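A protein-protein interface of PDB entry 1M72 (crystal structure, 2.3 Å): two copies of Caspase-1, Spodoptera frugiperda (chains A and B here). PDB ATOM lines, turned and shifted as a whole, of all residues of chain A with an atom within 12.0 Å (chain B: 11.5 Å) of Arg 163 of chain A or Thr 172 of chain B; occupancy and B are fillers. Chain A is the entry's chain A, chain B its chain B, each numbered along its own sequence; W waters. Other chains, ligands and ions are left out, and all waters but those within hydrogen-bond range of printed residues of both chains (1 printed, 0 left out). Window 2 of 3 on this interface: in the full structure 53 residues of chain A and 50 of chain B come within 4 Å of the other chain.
No position is printed for both chains.
Of the 26 pairs that touch across the chains among the printed residues, none has its exchanged pair printed and touching as well.
The backbone NH of Ile 159 of chain A lies within hydrogen-bond range of the backbone carbonyl oxygen of Ile 176 of chain B, at 2.8 Å.
The backbone carbonyl oxygen (O) of Leu 234 of chain A is in hydrogen-bond range of the guanidinium group (NH2) of Arg 20 of chain B (3.4 Å).
The backbone carbonyl oxygen of Ala 14 of chain B is in hydrogen-bond range of the backbone NH of Ser 162 of chain A (2.8 Å).
The backbone carbonyl oxygen (O) of Thr 160 of chain A lies within hydrogen-bond range of the backbone NH (N) of Ala 14 of chain B (2.9 Å).
The backbone carbonyl oxygen of Ser 162 of chain A sits at hydrogen-bond distance from the backbone NH of Met 16 of chain B (3.1 Å).
N of Arg 163 of chain A lies within hydrogen-bond range of O of Thr 172 of chain B, 3.2 Å away.
N of Leu 161 of chain A is in hydrogen-bond range of O of Tyr 174 of chain B (2.6 Å).
Water W1 lies within hydrogen-bond range of the backbone carbonyl oxygen of Leu 234 of chain A, the backbone carbonyl oxygen of Arg 175 of chain B and the guanidinium group of Arg 20 of chain B.
Arg 163 of chain A touches just these residues of chain B: Met 16 (3.8 Å) and Thr 172 (3.2 Å).
Thr 172 of chain B touches just these residues of chain A: Ser 162 (3.9 Å) and Arg 163 (3.2 Å).
Arg 15 of chain B touches just these residues of chain A: Leu 161 and Ser 162.
Of the printed residues of chain A, Met 16 of chain B touches Leu 161 (3.6 Å), Ser 162 (3.1 Å) and Arg 163 (3.8 Å).
Of the printed residues of chain A, Ala 139 of chain B touches Leu 161.
Of the printed residues of chain A, Ala 14 of chain B touches Ile 159, Thr 160, Leu 161 and Ser 162.
Val 18 of chain B touches none of the printed residues of chain A.
The nearest residue of chain B that does not touch Arg 163 of chain A is Ser 173 of chain B (5.0 Å).
Of the 18 printed residues of chain B, 12 touch a printed residue of chain A.
Hydrophobic or aromatic side chains of chain B that line the printed part of chain A: Val 13, Ala 14, Met 16, Pro 17, Ala 139, Tyr 174 and Ile 176.
Hydrophobic or aromatic side chains of chain A within 4 Å of the printed part of chain B: Ile 159, Leu 161 and Leu 234.
Among the printed residues, 26 pairs touch across the chains.
O of Arg 20 of chain B sits at hydrogen-bond distance from NH2 of Arg 261 of chain B, 2.8 Å away.
The side-chain hydroxyl (OH) of Tyr 174 of chain B is in hydrogen-bond range of the backbone carbonyl oxygen (O) of Val 18 of chain B, 2.6 Å away.
OH of Tyr 174 of chain B sits at hydrogen-bond distance from NH2 of Arg 261 of chain B.
The side-chain amide nitrogen of Asn 26 of chain B lies within hydrogen-bond range of the backbone carbonyl oxygen of Pro 17 of chain B (2.9 Å).
NE of Arg 20 of chain B lies within hydrogen-bond range of OD1 of Asn 21 of chain B (3.4 Å).
Among the printed residues, merely in contact across the chains: Thr 160 of chain A with Arg 175 of chain B (3.0 Å), Leu 161 of chain A with Ser 173 of chain B (3.0 Å), Ile 159 of chain A with Arg 175 of chain B (3.2 Å), Leu 161 of chain A with Ala 14 of chain B (3.3 Å), Ile 159 of chain A with Val 13 of chain B (3.5 Å), Thr 160 of chain A with Val 13 of chain B (3.5 Å), Ile 159 of chain A with Ala 14 of chain B (3.5 Å), Leu 234 of chain A with Tyr 174 of chain B (3.6 Å), Leu 161 of chain A with Met 16 of chain B (3.6 Å), Thr 160 of chain A with Tyr 174 of chain B (3.6 Å), Leu 161 of chain A with Arg 15 of chain B (3.6 Å), Ser 162 of chain A with Arg 15 of chain B (3.7 Å), Arg 163 of chain A with Met 16 of chain B (3.8 Å), Leu 234 of chain A with Ile 176 of chain B (3.8 Å), Leu 161 of chain A with Ala 139 of chain B (3.9 Å), Leu 161 of chain A with Pro 17 of chain B (3.9 Å), Ser 162 of chain A with Thr 172 of chain B (3.9 Å), Leu 234 of chain A with Arg 175 of chain B (3.96 Å) and Ser 162 of chain A with Ser 173 of chain B (3.9998 Å).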
ATOM      1  N   ILE A 159     -26.368   6.691  24.541  1.00  0.00           N
ATOM      2  CA  ILE A 159     -26.995   6.373  25.823  1.00  0.00           C
ATOM      3  C   ILE A 159     -25.936   5.726  26.749  1.00  0.00           C
ATOM      4  O   ILE A 159     -25.002   5.080  26.271  1.00  0.00           O
ATOM      5  CB  ILE A 159     -28.186   5.425  25.661  1.00  0.00           C
ATOM      6  CG1 ILE A 159     -28.913   5.272  27.005  1.00  0.00           C
ATOM      7  CG2 ILE A 159     -27.697   4.071  25.171  1.00  0.00           C
ATOM      8  CD1 ILE A 159     -30.308   4.634  26.911  1.00  0.00           C
ATOM      9  N   THR A 160     -26.086   5.905  28.062  1.00  0.00           N
ATOM     10  CA  THR A 160     -25.160   5.363  29.048  1.00  0.00           C
ATOM     11  C   THR A 160     -25.732   4.074  29.573  1.00  0.00           C
ATOM     12  O   THR A 160     -26.903   4.050  29.959  1.00  0.00           O
ATOM     13  CB  THR A 160     -24.982   6.328  30.248  1.00  0.00           C
ATOM     14  OG1 THR A 160     -24.302   7.501  29.808  1.00  0.00           O
ATOM     15  CG2 THR A 160     -24.158   5.676  31.382  1.00  0.00           C
ATOM     16  N   LEU A 161     -24.928   3.006  29.533  1.00  0.00           N
ATOM     17  CA  LEU A 161     -25.317   1.691  30.054  1.00  0.00           C
ATOM     18  C   LEU A 161     -24.665   1.625  31.420  1.00  0.00           C
ATOM     19  O   LEU A 161     -23.469   1.885  31.569  1.00  0.00           O
ATOM     20  CB  LEU A 161     -24.784   0.558  29.179  1.00  0.00           C
ATOM     21  CG  LEU A 161     -25.424   0.464  27.789  1.00  0.00           C
ATOM     22  CD1 LEU A 161     -24.967  -0.767  27.097  1.00  0.00           C
ATOM     23  CD2 LEU A 161     -26.929   0.495  27.934  1.00  0.00           C
ATOM     24  N   SER A 162     -25.452   1.282  32.425  1.00  0.00           N
ATOM     25  CA  SER A 162     -24.916   1.279  33.782  1.00  0.00           C
ATOM     26  C   SER A 162     -25.248   0.079  34.657  1.00  0.00           C
ATOM     27  O   SER A 162     -26.258  -0.603  34.437  1.00  0.00           O
ATOM     28  CB  SER A 162     -25.376   2.575  34.464  1.00  0.00           C
ATOM     29  OG  SER A 162     -25.034   2.612  35.827  1.00  0.00           O
ATOM     30  N   ARG A 163     -24.362  -0.143  35.644  1.00  0.00           N
ATOM     31  CA  ARG A 163     -24.432  -1.197  36.678  1.00  0.00           C
ATOM     32  C   ARG A 163     -24.031  -2.590  36.245  1.00  0.00           C
ATOM     33  O   ARG A 163     -23.007  -3.107  36.701  1.00  0.00           O
ATOM     34  CB  ARG A 163     -25.822  -1.241  37.321  1.00  0.00           C
ATOM     35  CG  ARG A 163     -26.114  -0.043  38.214  1.00  0.00           C
ATOM     36  CD  ARG A 163     -25.868  -0.382  39.674  1.00  0.00           C
ATOM     37  NE  ARG A 163     -27.125  -0.582  40.389  1.00  0.00           N
ATOM     38  CZ  ARG A 163     -28.140  -1.330  39.951  1.00  0.00           C
ATOM     39  NH1 ARG A 163     -28.075  -1.971  38.782  1.00  0.00           N
ATOM     40  NH2 ARG A 163     -29.238  -1.435  40.690  1.00  0.00           N
ATOM     41  N   LEU A 234     -17.674   2.251  21.068  1.00  0.00           N
ATOM     42  CA  LEU A 234     -17.278   2.366  22.466  1.00  0.00           C
ATOM     43  C   LEU A 234     -16.155   3.338  22.803  1.00  0.00           C
ATOM     44  O   LEU A 234     -16.234   4.015  23.797  1.00  0.00           O
ATOM     45  CB  LEU A 234     -16.892   0.973  23.030  1.00  0.00           C
ATOM     46  CG  LEU A 234     -17.992  -0.091  23.069  1.00  0.00           C
ATOM     47  CD1 LEU A 234     -17.477  -1.445  23.511  1.00  0.00           C
ATOM     48  CD2 LEU A 234     -19.047   0.382  24.002  1.00  0.00           C
ATOM     49  N   VAL B  13     -28.656   5.840  32.531  1.00  0.00           N
ATOM     50  CA  VAL B  13     -29.761   5.970  31.504  1.00  0.00           C
ATOM     51  C   VAL B  13     -30.408   4.595  31.189  1.00  0.00           C
ATOM     52  O   VAL B  13     -31.641   4.471  31.187  1.00  0.00           O
ATOM     53  CB  VAL B  13     -29.233   6.658  30.201  1.00  0.00           C
ATOM     54  N   ALA B  14     -29.601   3.565  30.944  1.00  0.00           N
ATOM     55  CA  ALA B  14     -30.148   2.229  30.688  1.00  0.00           C
ATOM     56  C   ALA B  14     -29.337   1.143  31.391  1.00  0.00           C
ATOM     57  O   ALA B  14     -28.172   1.349  31.752  1.00  0.00           O
ATOM     58  CB  ALA B  14     -30.190   1.946  29.169  1.00  0.00           C
ATOM     59  N   ARG B  15     -29.943  -0.018  31.583  1.00  0.00           N
ATOM     60  CA  ARG B  15     -29.233  -1.123  32.217  1.00  0.00           C
ATOM     61  C   ARG B  15     -28.179  -1.748  31.302  1.00  0.00           C
ATOM     62  O   ARG B  15     -28.419  -1.966  30.125  1.00  0.00           O
ATOM     63  CB  ARG B  15     -30.201  -2.234  32.636  1.00  0.00           C
ATOM     64  CG  ARG B  15     -29.503  -3.392  33.364  1.00  0.00           C
ATOM     65  CD  ARG B  15     -30.492  -4.464  33.801  1.00  0.00           C
ATOM     66  NE  ARG B  15     -31.697  -3.883  34.408  1.00  0.00           N
ATOM     67  CZ  ARG B  15     -32.708  -4.589  34.912  1.00  0.00           C
ATOM     68  NH1 ARG B  15     -32.675  -5.925  34.897  1.00  0.00           N
ATOM     69  NH2 ARG B  15     -33.769  -3.952  35.408  1.00  0.00           N
ATOM     70  N   MET B  16     -27.022  -2.065  31.865  1.00  0.00           N
ATOM     71  CA  MET B  16     -25.948  -2.690  31.132  1.00  0.00           C
ATOM     72  C   MET B  16     -26.284  -4.199  31.003  1.00  0.00           C
ATOM     73  O   MET B  16     -26.362  -4.913  31.994  1.00  0.00           O
ATOM     74  CB  MET B  16     -24.649  -2.462  31.918  1.00  0.00           C
ATOM     75  CG  MET B  16     -23.417  -3.073  31.298  1.00  0.00           C
ATOM     76  SD  MET B  16     -21.920  -2.894  32.325  1.00  0.00           S
ATOM     77  CE  MET B  16     -22.126  -1.169  32.809  1.00  0.00           C
ATOM     78  N   PRO B  17     -26.513  -4.696  29.774  1.00  0.00           N
ATOM     79  CA  PRO B  17     -26.844  -6.118  29.560  1.00  0.00           C
ATOM     80  C   PRO B  17     -25.645  -7.040  29.424  1.00  0.00           C
ATOM     81  O   PRO B  17     -25.791  -8.248  29.474  1.00  0.00           O
ATOM     82  CB  PRO B  17     -27.647  -6.098  28.267  1.00  0.00           C
ATOM     83  CG  PRO B  17     -26.920  -5.070  27.486  1.00  0.00           C
ATOM     84  CD  PRO B  17     -26.689  -3.931  28.529  1.00  0.00           C
ATOM     85  N   VAL B  18     -24.463  -6.466  29.252  1.00  0.00           N
ATOM     86  CA  VAL B  18     -23.267  -7.256  29.055  1.00  0.00           C
ATOM     87  C   VAL B  18     -22.078  -6.316  29.280  1.00  0.00           C
ATOM     88  O   VAL B  18     -22.201  -5.097  29.076  1.00  0.00           O
ATOM     89  CB  VAL B  18     -23.320  -7.843  27.623  1.00  0.00           C
ATOM     90  CG1 VAL B  18     -23.176  -6.735  26.582  1.00  0.00           C
ATOM     91  CG2 VAL B  18     -22.314  -8.937  27.468  1.00  0.00           C
ATOM     92  N   ASP B  19     -20.936  -6.837  29.716  1.00  0.00           N
ATOM     93  CA  ASP B  19     -19.824  -5.935  29.986  1.00  0.00           C
ATOM     94  C   ASP B  19     -19.293  -5.211  28.763  1.00  0.00           C
ATOM     95  O   ASP B  19     -19.393  -5.673  27.614  1.00  0.00           O
ATOM     96  CB  ASP B  19     -18.692  -6.630  30.725  1.00  0.00           C
ATOM     97  CG  ASP B  19     -18.155  -7.785  29.974  1.00  0.00           C
ATOM     98  OD1 ASP B  19     -18.928  -8.759  29.777  1.00  0.00           O
ATOM     99  OD2 ASP B  19     -16.962  -7.724  29.573  1.00  0.00           O
ATOM    100  N   ARG B  20     -18.703  -4.066  29.029  1.00  0.00           N
ATOM    101  CA  ARG B  20     -18.252  -3.219  27.970  1.00  0.00           C
ATOM    102  C   ARG B  20     -17.535  -3.844  26.785  1.00  0.00           C
ATOM    103  O   ARG B  20     -17.916  -3.598  25.621  1.00  0.00           O
ATOM    104  CB  ARG B  20     -17.409  -2.105  28.562  1.00  0.00           C
ATOM    105  CG  ARG B  20     -17.012  -1.053  27.558  1.00  0.00           C
ATOM    106  CD  ARG B  20     -15.850  -0.259  28.077  1.00  0.00           C
ATOM    107  NE  ARG B  20     -15.072   0.268  26.972  1.00  0.00           N
ATOM    108  CZ  ARG B  20     -14.962   1.555  26.723  1.00  0.00           C
ATOM    109  NH1 ARG B  20     -15.585   2.414  27.529  1.00  0.00           N
ATOM    110  NH2 ARG B  20     -14.261   1.982  25.674  1.00  0.00           N
ATOM    111  N   ASN B  21     -16.504  -4.642  27.060  1.00  0.00           N
ATOM    112  CA  ASN B  21     -15.695  -5.243  25.996  1.00  0.00           C
ATOM    113  C   ASN B  21     -15.986  -6.681  25.616  1.00  0.00           C
ATOM    114  O   ASN B  21     -15.141  -7.341  25.029  1.00  0.00           O
ATOM    115  CB  ASN B  21     -14.223  -5.135  26.359  1.00  0.00           C
ATOM    116  CG  ASN B  21     -13.833  -3.727  26.716  1.00  0.00           C
ATOM    117  OD1 ASN B  21     -14.039  -2.805  25.930  1.00  0.00           O
ATOM    118  ND2 ASN B  21     -13.283  -3.541  27.914  1.00  0.00           N
ATOM    119  N   ASN B  26     -24.911 -10.813  25.260  1.00  0.00           N
ATOM    120  CA  ASN B  26     -25.348 -11.706  26.328  1.00  0.00           C
ATOM    121  C   ASN B  26     -26.694 -12.268  25.925  1.00  0.00           C
ATOM    122  O   ASN B  26     -27.705 -11.588  25.978  1.00  0.00           O
ATOM    123  CB  ASN B  26     -25.448 -10.941  27.670  1.00  0.00           C
ATOM    124  CG  ASN B  26     -26.301 -11.685  28.750  1.00  0.00           C
ATOM    125  OD1 ASN B  26     -26.690 -12.841  28.575  1.00  0.00           O
ATOM    126  ND2 ASN B  26     -26.600 -10.992  29.856  1.00  0.00           N
ATOM    127  N   SER B  96     -36.408  -5.906  29.443  1.00  0.00           N
ATOM    128  CA  SER B  96     -35.347  -6.206  30.407  1.00  0.00           C
ATOM    129  C   SER B  96     -34.941  -7.666  30.464  1.00  0.00           C
ATOM    130  O   SER B  96     -33.757  -7.972  30.527  1.00  0.00           O
ATOM    131  CB  SER B  96     -35.753  -5.744  31.808  1.00  0.00           C
ATOM    132  OG  SER B  96     -35.816  -4.325  31.870  1.00  0.00           O
ATOM    133  N   ALA B 139     -31.507  -1.729  25.072  1.00  0.00           N
ATOM    134  CA  ALA B 139     -30.235  -1.052  24.862  1.00  0.00           C
ATOM    135  C   ALA B 139     -29.071  -2.013  25.115  1.00  0.00           C
ATOM    136  O   ALA B 139     -28.992  -2.669  26.164  1.00  0.00           O
ATOM    137  CB  ALA B 139     -30.112   0.189  25.767  1.00  0.00           C
ATOM    138  N   THR B 172     -18.047  -0.086  35.083  1.00  0.00           N
ATOM    139  CA  THR B 172     -19.048   0.583  35.925  1.00  0.00           C
ATOM    140  C   THR B 172     -20.225   1.108  35.080  1.00  0.00           C
ATOM    141  O   THR B 172     -21.420   0.991  35.458  1.00  0.00           O
ATOM    142  CB  THR B 172     -18.434   1.787  36.685  1.00  0.00           C
ATOM    143  OG1 THR B 172     -17.196   2.161  36.056  1.00  0.00           O
ATOM    144  CG2 THR B 172     -18.226   1.452  38.181  1.00  0.00           C
ATOM    145  N   SER B 173     -19.874   1.703  33.943  1.00  0.00           N
ATOM    146  CA  SER B 173     -20.868   2.241  33.038  1.00  0.00           C
ATOM    147  C   SER B 173     -20.121   2.637  31.784  1.00  0.00           C
ATOM    148  O   SER B 173     -18.958   3.052  31.847  1.00  0.00           O
ATOM    149  CB  SER B 173     -21.560   3.465  33.661  1.00  0.00           C
ATOM    150  OG  SER B 173     -20.775   4.639  33.509  1.00  0.00           O
ATOM    151  N   TYR B 174     -20.765   2.455  30.639  1.00  0.00           N
ATOM    152  CA  TYR B 174     -20.144   2.849  29.379  1.00  0.00           C
ATOM    153  C   TYR B 174     -21.262   3.332  28.449  1.00  0.00           C
ATOM    154  O   TYR B 174     -22.443   2.991  28.635  1.00  0.00           O
ATOM    155  CB  TYR B 174     -19.301   1.686  28.761  1.00  0.00           C
ATOM    156  CG  TYR B 174     -20.080   0.441  28.416  1.00  0.00           C
ATOM    157  CD1 TYR B 174     -20.676   0.289  27.155  1.00  0.00           C
ATOM    158  CD2 TYR B 174     -20.234  -0.587  29.350  1.00  0.00           C
ATOM    159  CE1 TYR B 174     -21.415  -0.876  26.841  1.00  0.00           C
ATOM    160  CE2 TYR B 174     -20.952  -1.747  29.055  1.00  0.00           C
ATOM    161  CZ  TYR B 174     -21.542  -1.897  27.800  1.00  0.00           C
ATOM    162  OH  TYR B 174     -22.221  -3.072  27.497  1.00  0.00           O
ATOM    163  N   ARG B 175     -20.886   4.156  27.476  1.00  0.00           N
ATOM    164  CA  ARG B 175     -21.848   4.729  26.535  1.00  0.00           C
ATOM    165  C   ARG B 175     -21.753   4.171  25.153  1.00  0.00           C
ATOM    166  O   ARG B 175     -20.652   3.940  24.653  1.00  0.00           O
ATOM    167  CB  ARG B 175     -21.693   6.250  26.467  1.00  0.00           C
ATOM    168  CG  ARG B 175     -22.342   6.897  27.639  1.00  0.00           C
ATOM    169  CD  ARG B 175     -21.886   8.316  27.817  1.00  0.00           C
ATOM    170  NE  ARG B 175     -22.003   9.074  26.581  1.00  0.00           N
ATOM    171  CZ  ARG B 175     -23.130   9.537  26.059  1.00  0.00           C
ATOM    172  NH1 ARG B 175     -24.298   9.335  26.657  1.00  0.00           N
ATOM    173  NH2 ARG B 175     -23.066  10.227  24.924  1.00  0.00           N
ATOM    174  N   ILE B 176     -22.925   3.989  24.536  1.00  0.00           N
ATOM    175  CA  ILE B 176     -23.029   3.457  23.173  1.00  0.00           C
ATOM    176  C   ILE B 176     -23.919   4.353  22.324  1.00  0.00           C
ATOM    177  O   ILE B 176     -24.688   5.151  22.859  1.00  0.00           O
ATOM    178  CB  ILE B 176     -23.628   2.030  23.176  1.00  0.00           C
ATOM    179  CG1 ILE B 176     -25.080   2.074  23.710  1.00  0.00           C
ATOM    180  CG2 ILE B 176     -22.729   1.114  24.031  1.00  0.00           C
ATOM    181  CD1 ILE B 176     -25.983   0.832  23.357  1.00  0.00           C
ATOM    182  N   ARG B 261     -21.178  -6.472  18.530  1.00  0.00           N
ATOM    183  CA  ARG B 261     -20.677  -7.693  19.121  1.00  0.00           C
ATOM    184  C   ARG B 261     -21.175  -8.850  18.243  1.00  0.00           C
ATOM    185  O   ARG B 261     -22.008  -8.655  17.355  1.00  0.00           O
ATOM    186  CB  ARG B 261     -21.190  -7.863  20.563  1.00  0.00           C
ATOM    187  CG  ARG B 261     -20.985  -6.635  21.464  1.00  0.00           C
ATOM    188  CD  ARG B 261     -21.434  -6.956  22.874  1.00  0.00           C
ATOM    189  NE  ARG B 261     -21.492  -5.751  23.700  1.00  0.00           N
ATOM    190  CZ  ARG B 261     -20.423  -5.048  24.084  1.00  0.00           C
ATOM    191  NH1 ARG B 261     -19.176  -5.426  23.743  1.00  0.00           N
ATOM    192  NH2 ARG B 261     -20.605  -3.927  24.765  1.00  0.00           N
HETATM  193  O   HOH W   1     -18.096   3.553  25.856  1.00  0.00           O
